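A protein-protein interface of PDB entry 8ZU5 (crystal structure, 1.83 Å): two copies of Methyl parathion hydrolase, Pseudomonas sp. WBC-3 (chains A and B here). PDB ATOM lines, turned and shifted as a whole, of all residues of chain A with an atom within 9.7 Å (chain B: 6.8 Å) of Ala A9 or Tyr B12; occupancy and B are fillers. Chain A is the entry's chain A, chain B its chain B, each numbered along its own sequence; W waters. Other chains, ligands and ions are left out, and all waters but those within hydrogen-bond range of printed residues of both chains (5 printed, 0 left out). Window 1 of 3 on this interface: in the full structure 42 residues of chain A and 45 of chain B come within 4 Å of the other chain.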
ATOM      1  N   VAL A   5      18.686   6.462  14.418  1.00  0.00           N
ATOM      2  CA  VAL A   5      18.504   5.063  14.064  1.00  0.00           C
ATOM      3  C   VAL A   5      19.801   4.292  14.284  1.00  0.00           C
ATOM      4  O   VAL A   5      19.804   3.197  14.867  1.00  0.00           O
ATOM      5  CB  VAL A   5      18.007   4.956  12.611  1.00  0.00           C
ATOM      6  CG1 VAL A   5      17.707   3.508  12.247  1.00  0.00           C
ATOM      7  CG2 VAL A   5      16.786   5.825  12.423  1.00  0.00           C
ATOM      8  N   ARG A   6      20.921   4.877  13.854  1.00  0.00           N
ATOM      9  CA  ARG A   6      22.245   4.266  13.920  1.00  0.00           C
ATOM     10  C   ARG A   6      22.204   2.787  13.536  1.00  0.00           C
ATOM     11  O   ARG A   6      22.686   1.909  14.257  1.00  0.00           O
ATOM     12  CB  ARG A   6      22.900   4.476  15.296  1.00  0.00           C
ATOM     13  CG  ARG A   6      23.382   5.911  15.523  1.00  0.00           C
ATOM     14  CD  ARG A   6      24.127   6.108  16.840  1.00  0.00           C
ATOM     15  NE  ARG A   6      24.597   7.487  16.967  1.00  0.00           N
ATOM     16  CZ  ARG A   6      25.253   7.979  18.012  1.00  0.00           C
ATOM     17  NH1 ARG A   6      25.503   7.244  19.082  1.00  0.00           N
ATOM     18  NH2 ARG A   6      25.661   9.245  17.984  1.00  0.00           N
ATOM     19  N   THR A   7      21.618   2.520  12.367  1.00  0.00           N
ATOM     20  CA  THR A   7      21.650   1.197  11.746  1.00  0.00           C
ATOM     21  C   THR A   7      22.064   1.362  10.293  1.00  0.00           C
ATOM     22  O   THR A   7      21.436   2.126   9.552  1.00  0.00           O
ATOM     23  CB  THR A   7      20.287   0.477  11.838  1.00  0.00           C
ATOM     24  OG1 THR A   7      19.332   1.119  10.981  1.00  0.00           O
ATOM     25  CG2 THR A   7      19.758   0.470  13.262  1.00  0.00           C
ATOM     26  N   SER A   8      23.125   0.659   9.899  1.00  0.00           N
ATOM     27  CA  SER A   8      23.602   0.713   8.527  1.00  0.00           C
ATOM     28  C   SER A   8      22.605   0.063   7.571  1.00  0.00           C
ATOM     29  O   SER A   8      21.866  -0.858   7.929  1.00  0.00           O
ATOM     30  CB  SER A   8      24.956   0.003   8.401  1.00  0.00           C
ATOM     31  OG  SER A   8      25.989   0.751   9.010  1.00  0.00           O
ATOM     32  N   ALA A   9      22.610   0.545   6.335  1.00  0.00           N
ATOM     33  CA  ALA A   9      21.895  -0.042   5.211  1.00  0.00           C
ATOM     34  C   ALA A   9      22.187  -1.538   5.133  1.00  0.00           C
ATOM     35  O   ALA A   9      23.240  -1.976   5.617  1.00  0.00           O
ATOM     36  CB  ALA A   9      22.330   0.656   3.917  1.00  0.00           C
ATOM     37  N   PRO A  10      21.322  -2.348   4.518  1.00  0.00           N
ATOM     38  CA  PRO A  10      21.683  -3.760   4.340  1.00  0.00           C
ATOM     39  C   PRO A  10      22.977  -3.868   3.560  1.00  0.00           C
ATOM     40  O   PRO A  10      23.212  -3.132   2.605  1.00  0.00           O
ATOM     41  CB  PRO A  10      20.502  -4.357   3.564  1.00  0.00           C
ATOM     42  CG  PRO A  10      19.692  -3.199   3.060  1.00  0.00           C
ATOM     43  CD  PRO A  10      20.270  -1.919   3.577  1.00  0.00           C
ATOM     44  N   GLY A  11      23.824  -4.786   3.993  1.00  0.00           N
ATOM     45  CA  GLY A  11      25.066  -5.010   3.309  1.00  0.00           C
ATOM     46  C   GLY A  11      24.910  -5.853   2.064  1.00  0.00           C
ATOM     47  O   GLY A  11      25.352  -7.005   2.038  1.00  0.00           O
ATOM     48  N   TYR A  12      24.290  -5.303   1.020  1.00  0.00           N
ATOM     49  CA  TYR A  12      24.445  -5.891  -0.301  1.00  0.00           C
ATOM     50  C   TYR A  12      24.562  -4.752  -1.302  1.00  0.00           C
ATOM     51  O   TYR A  12      24.124  -3.625  -1.042  1.00  0.00           O
ATOM     52  CB  TYR A  12      23.316  -6.902  -0.638  1.00  0.00           C
ATOM     53  CG  TYR A  12      21.922  -6.333  -0.835  1.00  0.00           C
ATOM     54  CD1 TYR A  12      21.088  -6.107   0.252  1.00  0.00           C
ATOM     55  CD2 TYR A  12      21.458  -6.013  -2.108  1.00  0.00           C
ATOM     56  CE1 TYR A  12      19.810  -5.605   0.074  1.00  0.00           C
ATOM     57  CE2 TYR A  12      20.182  -5.515  -2.303  1.00  0.00           C
ATOM     58  CZ  TYR A  12      19.365  -5.309  -1.207  1.00  0.00           C
ATOM     59  OH  TYR A  12      18.116  -4.774  -1.398  1.00  0.00           O
ATOM     60  N   TYR A  13      25.260  -5.040  -2.399  1.00  0.00           N
ATOM     61  CA  TYR A  13      25.562  -4.054  -3.437  1.00  0.00           C
ATOM     62  C   TYR A  13      25.415  -4.726  -4.793  1.00  0.00           C
ATOM     63  O   TYR A  13      26.081  -5.728  -5.062  1.00  0.00           O
ATOM     64  CB  TYR A  13      26.976  -3.492  -3.290  1.00  0.00           C
ATOM     65  CG  TYR A  13      27.289  -2.365  -4.227  1.00  0.00           C
ATOM     66  CD1 TYR A  13      27.811  -2.617  -5.488  1.00  0.00           C
ATOM     67  CD2 TYR A  13      27.068  -1.027  -3.848  1.00  0.00           C
ATOM     68  CE1 TYR A  13      28.114  -1.572  -6.359  1.00  0.00           C
ATOM     69  CE2 TYR A  13      27.359   0.014  -4.704  1.00  0.00           C
ATOM     70  CZ  TYR A  13      27.906  -0.268  -5.952  1.00  0.00           C
ATOM     71  OH  TYR A  13      28.202   0.756  -6.824  1.00  0.00           O
ATOM     72  N   SER A  26      27.932  -8.270   2.215  1.00  0.00           N
ATOM     73  CA  SER A  26      28.757  -7.945   3.369  1.00  0.00           C
ATOM     74  C   SER A  26      28.586  -9.001   4.457  1.00  0.00           C
ATOM     75  O   SER A  26      27.471  -9.434   4.744  1.00  0.00           O
ATOM     76  CB  SER A  26      28.388  -6.569   3.918  1.00  0.00           C
ATOM     77  OG  SER A  26      29.124  -6.338   5.089  1.00  0.00           O
ATOM     78  N   GLY A  28      29.979  -8.183   7.396  1.00  0.00           N
ATOM     79  CA  GLY A  28      30.267  -7.321   8.514  1.00  0.00           C
ATOM     80  C   GLY A  28      31.640  -6.715   8.349  1.00  0.00           C
ATOM     81  O   GLY A  28      32.237  -6.757   7.267  1.00  0.00           O
ATOM     82  N   ARG A  90      27.334 -11.754   8.975  1.00  0.00           N
ATOM     83  CA  ARG A  90      26.150 -11.091   8.433  1.00  0.00           C
ATOM     84  C   ARG A  90      25.759 -11.620   7.056  1.00  0.00           C
ATOM     85  O   ARG A  90      24.686 -11.265   6.554  1.00  0.00           O
ATOM     86  CB  ARG A  90      26.395  -9.585   8.334  1.00  0.00           C
ATOM     87  CG  ARG A  90      26.041  -8.764   9.563  1.00  0.00           C
ATOM     88  CD  ARG A  90      26.278  -9.530  10.834  1.00  0.00           C
ATOM     89  NE  ARG A  90      26.531  -8.642  11.962  1.00  0.00           N
ATOM     90  CZ  ARG A  90      27.146  -9.013  13.076  1.00  0.00           C
ATOM     91  NH1 ARG A  90      27.584 -10.249  13.245  1.00  0.00           N
ATOM     92  NH2 ARG A  90      27.339  -8.117  14.039  1.00  0.00           N
ATOM     93  N   ASN A  94      22.244 -11.042   4.702  1.00  0.00           N
ATOM     94  CA  ASN A  94      22.371 -10.123   3.572  1.00  0.00           C
ATOM     95  C   ASN A  94      22.142 -10.807   2.225  1.00  0.00           C
ATOM     96  O   ASN A  94      21.678 -10.161   1.284  1.00  0.00           O
ATOM     97  CB  ASN A  94      23.734  -9.408   3.602  1.00  0.00           C
ATOM     98  CG  ASN A  94      23.790  -8.362   4.703  1.00  0.00           C
ATOM     99  OD1 ASN A  94      22.752  -7.737   5.016  1.00  0.00           O
ATOM    100  ND2 ASN A  94      24.979  -8.128   5.274  1.00  0.00           N
ATOM    101  N   ALA A  97      18.476 -10.419   2.235  1.00  0.00           N
ATOM    102  CA  ALA A  97      18.126  -9.051   1.869  1.00  0.00           C
ATOM    103  C   ALA A  97      18.294  -8.815   0.372  1.00  0.00           C
ATOM    104  O   ALA A  97      17.537  -8.045  -0.228  1.00  0.00           O
ATOM    105  CB  ALA A  97      18.982  -8.059   2.665  1.00  0.00           C
ATOM    106  N   PHE A 270      33.954  -2.308   1.735  1.00  0.00           N
ATOM    107  CA  PHE A 270      32.762  -2.850   1.087  1.00  0.00           C
ATOM    108  C   PHE A 270      32.150  -1.792   0.163  1.00  0.00           C
ATOM    109  O   PHE A 270      32.008  -0.631   0.578  1.00  0.00           O
ATOM    110  CB  PHE A 270      31.730  -3.268   2.148  1.00  0.00           C
ATOM    111  CG  PHE A 270      30.478  -3.814   1.563  1.00  0.00           C
ATOM    112  CD1 PHE A 270      30.461  -5.106   1.114  1.00  0.00           C
ATOM    113  CD2 PHE A 270      29.328  -3.052   1.467  1.00  0.00           C
ATOM    114  CE1 PHE A 270      29.305  -5.655   0.523  1.00  0.00           C
ATOM    115  CE2 PHE A 270      28.156  -3.588   0.892  1.00  0.00           C
ATOM    116  CZ  PHE A 270      28.143  -4.881   0.429  1.00  0.00           C
ATOM    117  N   TYR A 290      29.161   4.439  -8.723  1.00  0.00           N
ATOM    118  CA  TYR A 290      27.840   3.983  -8.283  1.00  0.00           C
ATOM    119  C   TYR A 290      26.880   4.002  -9.466  1.00  0.00           C
ATOM    120  O   TYR A 290      26.852   4.962 -10.242  1.00  0.00           O
ATOM    121  CB  TYR A 290      27.290   4.853  -7.131  1.00  0.00           C
ATOM    122  CG  TYR A 290      25.883   4.434  -6.703  1.00  0.00           C
ATOM    123  CD1 TYR A 290      25.678   3.296  -5.925  1.00  0.00           C
ATOM    124  CD2 TYR A 290      24.748   5.199  -7.068  1.00  0.00           C
ATOM    125  CE1 TYR A 290      24.361   2.897  -5.534  1.00  0.00           C
ATOM    126  CE2 TYR A 290      23.428   4.814  -6.669  1.00  0.00           C
ATOM    127  CZ  TYR A 290      23.254   3.666  -5.911  1.00  0.00           C
ATOM    128  OH  TYR A 290      21.972   3.282  -5.543  1.00  0.00           O
ATOM    129  N   ALA B   9      20.293  -2.033  -3.910  1.00  0.00           N
ATOM    130  CA  ALA B   9      19.919  -1.954  -2.504  1.00  0.00           C
ATOM    131  C   ALA B   9      19.328  -0.568  -2.249  1.00  0.00           C
ATOM    132  O   ALA B   9      19.558   0.355  -3.028  1.00  0.00           O
ATOM    133  CB  ALA B   9      21.137  -2.194  -1.601  1.00  0.00           C
ATOM    134  N   PRO B  10      18.530  -0.398  -1.197  1.00  0.00           N
ATOM    135  CA  PRO B  10      18.011   0.945  -0.911  1.00  0.00           C
ATOM    136  C   PRO B  10      19.170   1.931  -0.816  1.00  0.00           C
ATOM    137  O   PRO B  10      20.245   1.617  -0.286  1.00  0.00           O
ATOM    138  CB  PRO B  10      17.273   0.772   0.425  1.00  0.00           C
ATOM    139  CG  PRO B  10      16.962  -0.700   0.492  1.00  0.00           C
ATOM    140  CD  PRO B  10      18.096  -1.394  -0.206  1.00  0.00           C
ATOM    141  N   GLY B  11      18.980   3.095  -1.436  1.00  0.00           N
ATOM    142  CA  GLY B  11      20.031   4.079  -1.544  1.00  0.00           C
ATOM    143  C   GLY B  11      20.110   4.990  -0.339  1.00  0.00           C
ATOM    144  O   GLY B  11      19.737   6.164  -0.420  1.00  0.00           O
ATOM    145  N   TYR B  12      20.567   4.450   0.789  1.00  0.00           N
ATOM    146  CA  TYR B  12      20.946   5.268   1.926  1.00  0.00           C
ATOM    147  C   TYR B  12      22.210   4.697   2.544  1.00  0.00           C
ATOM    148  O   TYR B  12      22.437   3.485   2.520  1.00  0.00           O
ATOM    149  CB  TYR B  12      19.807   5.367   2.959  1.00  0.00           C
ATOM    150  CG  TYR B  12      19.450   4.086   3.690  1.00  0.00           C
ATOM    151  CD1 TYR B  12      18.520   3.172   3.163  1.00  0.00           C
ATOM    152  CD2 TYR B  12      20.038   3.791   4.912  1.00  0.00           C
ATOM    153  CE1 TYR B  12      18.192   2.007   3.845  1.00  0.00           C
ATOM    154  CE2 TYR B  12      19.717   2.636   5.600  1.00  0.00           C
ATOM    155  CZ  TYR B  12      18.803   1.745   5.065  1.00  0.00           C
ATOM    156  OH  TYR B  12      18.521   0.607   5.787  1.00  0.00           O
ATOM    157  N   TYR B  13      23.024   5.582   3.113  1.00  0.00           N
ATOM    158  CA  TYR B  13      24.314   5.207   3.695  1.00  0.00           C
ATOM    159  C   TYR B  13      24.529   5.943   5.009  1.00  0.00           C
ATOM    160  O   TYR B  13      24.541   7.170   5.017  1.00  0.00           O
ATOM    161  CB  TYR B  13      25.442   5.544   2.730  1.00  0.00           C
ATOM    162  CG  TYR B  13      26.785   5.069   3.161  1.00  0.00           C
ATOM    163  CD1 TYR B  13      27.547   5.814   4.076  1.00  0.00           C
ATOM    164  CD2 TYR B  13      27.358   3.928   2.575  1.00  0.00           C
ATOM    165  CE1 TYR B  13      28.798   5.385   4.464  1.00  0.00           C
ATOM    166  CE2 TYR B  13      28.628   3.508   2.936  1.00  0.00           C
ATOM    167  CZ  TYR B  13      29.338   4.230   3.865  1.00  0.00           C
ATOM    168  OH  TYR B  13      30.601   3.792   4.205  1.00  0.00           O
ATOM    169  N   ARG B  14      24.747   5.192   6.097  1.00  0.00           N
ATOM    170  CA  ARG B  14      24.746   5.702   7.468  1.00  0.00           C
ATOM    171  C   ARG B  14      26.170   5.892   7.967  1.00  0.00           C
ATOM    172  O   ARG B  14      27.025   5.025   7.749  1.00  0.00           O
ATOM    173  CB  ARG B  14      24.036   4.726   8.412  1.00  0.00           C
ATOM    174  CG  ARG B  14      23.546   5.314   9.718  1.00  0.00           C
ATOM    175  CD  ARG B  14      22.157   5.835   9.569  1.00  0.00           C
ATOM    176  NE  ARG B  14      21.214   4.736   9.418  1.00  0.00           N
ATOM    177  CZ  ARG B  14      19.935   4.887   9.106  1.00  0.00           C
ATOM    178  NH1 ARG B  14      19.400   6.092   8.940  1.00  0.00           N
ATOM    179  NH2 ARG B  14      19.182   3.805   8.934  1.00  0.00           N
ATOM    180  N   THR B  23      23.077  10.437   7.243  1.00  0.00           N
ATOM    181  CA  THR B  23      22.544   9.487   6.283  1.00  0.00           C
ATOM    182  C   THR B  23      22.605  10.150   4.917  1.00  0.00           C
ATOM    183  O   THR B  23      21.815  11.053   4.635  1.00  0.00           O
ATOM    184  CB  THR B  23      21.108   9.053   6.608  1.00  0.00           C
ATOM    185  OG1 THR B  23      21.021   8.632   7.979  1.00  0.00           O
ATOM    186  CG2 THR B  23      20.752   7.864   5.707  1.00  0.00           C
ATOM    187  N   ALA B  24      23.551   9.726   4.082  1.00  0.00           N
ATOM    188  CA  ALA B  24      23.505  10.095   2.677  1.00  0.00           C
ATOM    189  C   ALA B  24      22.268   9.435   2.062  1.00  0.00           C
ATOM    190  O   ALA B  24      22.059   8.231   2.240  1.00  0.00           O
ATOM    191  CB  ALA B  24      24.781   9.619   1.964  1.00  0.00           C
ATOM    192  N   LEU B  25      21.464  10.208   1.329  1.00  0.00           N
ATOM    193  CA  LEU B  25      20.229   9.724   0.714  1.00  0.00           C
ATOM    194  C   LEU B  25      20.333   9.873  -0.797  1.00  0.00           C
ATOM    195  O   LEU B  25      20.446  10.993  -1.310  1.00  0.00           O
ATOM    196  CB  LEU B  25      18.992  10.475   1.236  1.00  0.00           C
ATOM    197  CG  LEU B  25      18.654  10.387   2.725  1.00  0.00           C
ATOM    198  CD1 LEU B  25      17.543  11.371   3.109  1.00  0.00           C
ATOM    199  CD2 LEU B  25      18.203   8.971   3.114  1.00  0.00           C
ATOM    200  N   SER B  26      20.273   8.752  -1.508  1.00  0.00           N
ATOM    201  CA  SER B  26      20.410   8.799  -2.958  1.00  0.00           C
ATOM    202  C   SER B  26      19.096   9.174  -3.618  1.00  0.00           C
ATOM    203  O   SER B  26      18.042   8.601  -3.300  1.00  0.00           O
ATOM    204  CB  SER B  26      20.883   7.459  -3.509  1.00  0.00           C
ATOM    205  OG  SER B  26      20.940   7.543  -4.924  1.00  0.00           O
ATOM    206  N   ALA B  93      11.744   7.896  -1.207  1.00  0.00           N
ATOM    207  CA  ALA B  93      11.663   6.489  -0.855  1.00  0.00           C
ATOM    208  C   ALA B  93      12.844   6.069   0.001  1.00  0.00           C
ATOM    209  O   ALA B  93      12.682   5.278   0.941  1.00  0.00           O
ATOM    210  CB  ALA B  93      11.581   5.627  -2.114  1.00  0.00           C
ATOM    211  N   ASN B  94      14.056   6.569  -0.334  1.00  0.00           N
ATOM    212  CA  ASN B  94      15.258   6.227   0.419  1.00  0.00           C
ATOM    213  C   ASN B  94      15.289   6.871   1.805  1.00  0.00           C
ATOM    214  O   ASN B  94      15.830   6.284   2.750  1.00  0.00           O
ATOM    215  CB  ASN B  94      16.499   6.611  -0.398  1.00  0.00           C
ATOM    216  CG  ASN B  94      16.716   5.665  -1.547  1.00  0.00           C
ATOM    217  OD1 ASN B  94      16.450   4.480  -1.390  1.00  0.00           O
ATOM    218  ND2 ASN B  94      17.273   6.150  -2.674  1.00  0.00           N
ATOM    219  N   LEU B  95      14.718   8.067   1.955  1.00  0.00           N
ATOM    220  CA  LEU B  95      14.464   8.601   3.283  1.00  0.00           C
ATOM    221  C   LEU B  95      13.615   7.633   4.103  1.00  0.00           C
ATOM    222  O   LEU B  95      13.963   7.295   5.240  1.00  0.00           O
ATOM    223  CB  LEU B  95      13.773   9.966   3.177  1.00  0.00           C
ATOM    224  CG  LEU B  95      13.301  10.576   4.496  1.00  0.00           C
ATOM    225  CD1 LEU B  95      14.484  10.578   5.415  1.00  0.00           C
ATOM    226  CD2 LEU B  95      12.744  11.999   4.304  1.00  0.00           C
ATOM    227  N   LYS B  96      12.512   7.141   3.532  1.00  0.00           N
ATOM    228  CA  LYS B  96      11.700   6.192   4.306  1.00  0.00           C
ATOM    229  C   LYS B  96      12.441   4.878   4.566  1.00  0.00           C
ATOM    230  O   LYS B  96      12.371   4.340   5.679  1.00  0.00           O
ATOM    231  CB  LYS B  96      10.351   5.949   3.625  1.00  0.00           C
ATOM    232  CG  LYS B  96       9.630   7.258   3.296  1.00  0.00           C
ATOM    233  CD  LYS B  96       8.217   7.038   2.854  1.00  0.00           C
ATOM    234  CE  LYS B  96       8.255   6.408   1.477  1.00  0.00           C
ATOM    235  NZ  LYS B  96       8.100   7.409   0.364  1.00  0.00           N
ATOM    236  N   ALA B  97      13.170   4.354   3.569  1.00  0.00           N
ATOM    237  CA  ALA B  97      13.890   3.097   3.761  1.00  0.00           C
ATOM    238  C   ALA B  97      14.989   3.238   4.804  1.00  0.00           C
ATOM    239  O   ALA B  97      15.360   2.257   5.458  1.00  0.00           O
ATOM    240  CB  ALA B  97      14.462   2.606   2.433  1.00  0.00           C
ATOM    241  N   ALA B  98      15.516   4.439   4.984  1.00  0.00           N
ATOM    242  CA  ALA B  98      16.456   4.727   6.058  1.00  0.00           C
ATOM    243  C   ALA B  98      15.788   4.853   7.426  1.00  0.00           C
ATOM    244  O   ALA B  98      16.481   5.192   8.388  1.00  0.00           O
ATOM    245  CB  ALA B  98      17.236   6.020   5.759  1.00  0.00           C
ATOM    246  N   GLY B  99      14.472   4.627   7.532  1.00  0.00           N
ATOM    247  CA  GLY B  99      13.789   4.586   8.820  1.00  0.00           C
ATOM    248  C   GLY B  99      13.290   5.907   9.355  1.00  0.00           C
ATOM    249  O   GLY B  99      13.134   6.049  10.571  1.00  0.00           O
ATOM    250  N   PHE B 270      27.819   8.079  -5.220  1.00  0.00           N
ATOM    251  CA  PHE B 270      27.087   7.890  -3.972  1.00  0.00           C
ATOM    252  C   PHE B 270      27.842   6.901  -3.085  1.00  0.00           C
ATOM    253  O   PHE B 270      28.321   5.870  -3.580  1.00  0.00           O
ATOM    254  CB  PHE B 270      25.675   7.361  -4.278  1.00  0.00           C
ATOM    255  CG  PHE B 270      24.874   7.025  -3.062  1.00  0.00           C
ATOM    256  CD1 PHE B 270      24.176   8.029  -2.391  1.00  0.00           C
ATOM    257  CD2 PHE B 270      24.835   5.732  -2.587  1.00  0.00           C
ATOM    258  CE1 PHE B 270      23.459   7.760  -1.250  1.00  0.00           C
ATOM    259  CE2 PHE B 270      24.108   5.427  -1.448  1.00  0.00           C
ATOM    260  CZ  PHE B 270      23.410   6.455  -0.772  1.00  0.00           C
ATOM    261  N   PRO B 271      27.963   7.152  -1.774  1.00  0.00           N
ATOM    262  CA  PRO B 271      27.364   8.211  -0.952  1.00  0.00           C
ATOM    263  C   PRO B 271      28.083   9.575  -1.019  1.00  0.00           C
ATOM    264  O   PRO B 271      27.628  10.562  -0.434  1.00  0.00           O
ATOM    265  CB  PRO B 271      27.466   7.624   0.468  1.00  0.00           C
ATOM    266  CG  PRO B 271      28.793   6.845   0.412  1.00  0.00           C
ATOM    267  CD  PRO B 271      28.735   6.191  -0.952  1.00  0.00           C
ATOM    268  N   TYR B 290      34.250   2.010   4.671  1.00  0.00           N
ATOM    269  CA  TYR B 290      32.984   1.431   5.094  1.00  0.00           C
ATOM    270  C   TYR B 290      33.059   1.092   6.569  1.00  0.00           C
ATOM    271  O   TYR B 290      34.012   0.454   7.031  1.00  0.00           O
ATOM    272  CB  TYR B 290      32.672   0.160   4.302  1.00  0.00           C
ATOM    273  CG  TYR B 290      31.349  -0.513   4.668  1.00  0.00           C
ATOM    274  CD1 TYR B 290      30.137  -0.008   4.221  1.00  0.00           C
ATOM    275  CD2 TYR B 290      31.319  -1.635   5.489  1.00  0.00           C
ATOM    276  CE1 TYR B 290      28.932  -0.624   4.548  1.00  0.00           C
ATOM    277  CE2 TYR B 290      30.112  -2.240   5.849  1.00  0.00           C
ATOM    278  CZ  TYR B 290      28.935  -1.741   5.367  1.00  0.00           C
ATOM    279  OH  TYR B 290      27.749  -2.353   5.719  1.00  0.00           O
HETATM  280  O   HOH W   1      20.023   5.202  -5.991  1.00  0.00           O
HETATM  281  O   HOH W   2      27.846  -4.814   6.804  1.00  0.00           O
HETATM  282  O   HOH W   3      27.082   2.240   7.271  1.00  0.00           O
HETATM  283  O   HOH W   4      21.970   1.656  -3.676  1.00  0.00           O
HETATM  284  O   HOH W   5      24.896   2.318   5.884  1.00  0.00           O
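Printed residues of chain A that touch a printed residue of chain B: Val A5, Thr A7, Ala A9, Pro A10, Tyr A12, Phe A270 and Tyr A290.
Hydrophobic or aromatic side chains of chain A that line the printed part of chain B: Val A5, Ala A9, Pro A10, Tyr A12, Phe A270 and Tyr A290.
Hydrophobic or aromatic side chains of chain B within 4 Å of the printed part of chain A: Ala B9, Pro B10, Tyr B12, Phe B270 and Tyr B290.
Among the printed residues, no Asp or Glu carboxylate lies within 4 Å of a Lys or Arg side-chain nitrogen of the other chain.
Water W4 bridges OH of Tyr A290 and O of Ala B9.
Water W3 bridges the side-chain hydroxyl (OG) of Ser A8 (2.5 Å) and the backbone carbonyl oxygen (O) of Arg B14 (2.8 Å).
Water W2 bridges OG of Ser A26 (2.6 Å) and OH of Tyr B290 (2.7 Å).
Water W1 bridges OG of Ser B26 (2.7 Å) and OH of Tyr A290 (2.8 Å).
Water W5 lies within hydrogen-bond range of N of Arg B14 (2.9 Å) and N of Ala A9 (2.9 Å).
Ala A9 touches just one residue of chain B: Tyr B12 (3.2 Å).
Of the printed residues of chain A, Tyr B12 touches Ala A9 (3.2 Å) and Pro A10 (3.8 Å).
No residue of chain A comes within 4 Å of Ala B24.
Ala B97 touches none of the printed residues of chain A.
No residue of chain A comes within 4 Å of Ala B98.
Printed residues of chain B within 4 Å of Pro A10: Tyr B12 (3.8 Å).
Printed residues of chain A within 4 Å of Phe B270: Tyr A290.
The nearest residue of chain B that does not touch Ala A9 is Tyr B290 (4.5 Å).
The nearest residue of chain A that does not touch Tyr B12 is Ser A8 (4.2 Å).
The guanidinium group (NE) of Arg B14 sits at hydrogen-bond distance from the backbone carbonyl oxygen (O) of Thr A7, at 2.6 Å.
OG1 of Thr B23 sits at hydrogen-bond distance from NH1 of Arg B14, at 3.2 Å.
The guanidinium group of Arg B14 sits at hydrogen-bond distance from the backbone carbonyl oxygen of Ala B98, 3.1 Å away.
Ala A9 touches Tyr B12, and with the chains exchanged Tyr A12 touches Ala B9.
Pro A10 touches Tyr B12, and with the chains exchanged Tyr A12 touches Pro B10.
Phe A270 touches Tyr B290, and with the chains exchanged Tyr A290 touches Phe B270.
10 positions are printed for both chains.
Of the 8 pairs that touch across the chains among the printed residues, 6 have their exchanged pair printed and touching as well.
CG1 of Val A5 touches NH2 of Arg B14, 3.6 Å away.
Ala A9 touches Tyr B12 (CB to O, 3.2 Å).
OH of Tyr B12 touches CD of Pro A10 (3.8 Å).
Tyr A12 touches Ala B9 (O to CB, 3.4 Å).
Tyr A12 touches Pro B10.
CB of Phe A270 touches CD2 of Tyr B290, at 3.7 Å.
Tyr A290 touches Phe B270 (CD2 to CB, 3.6 Å).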
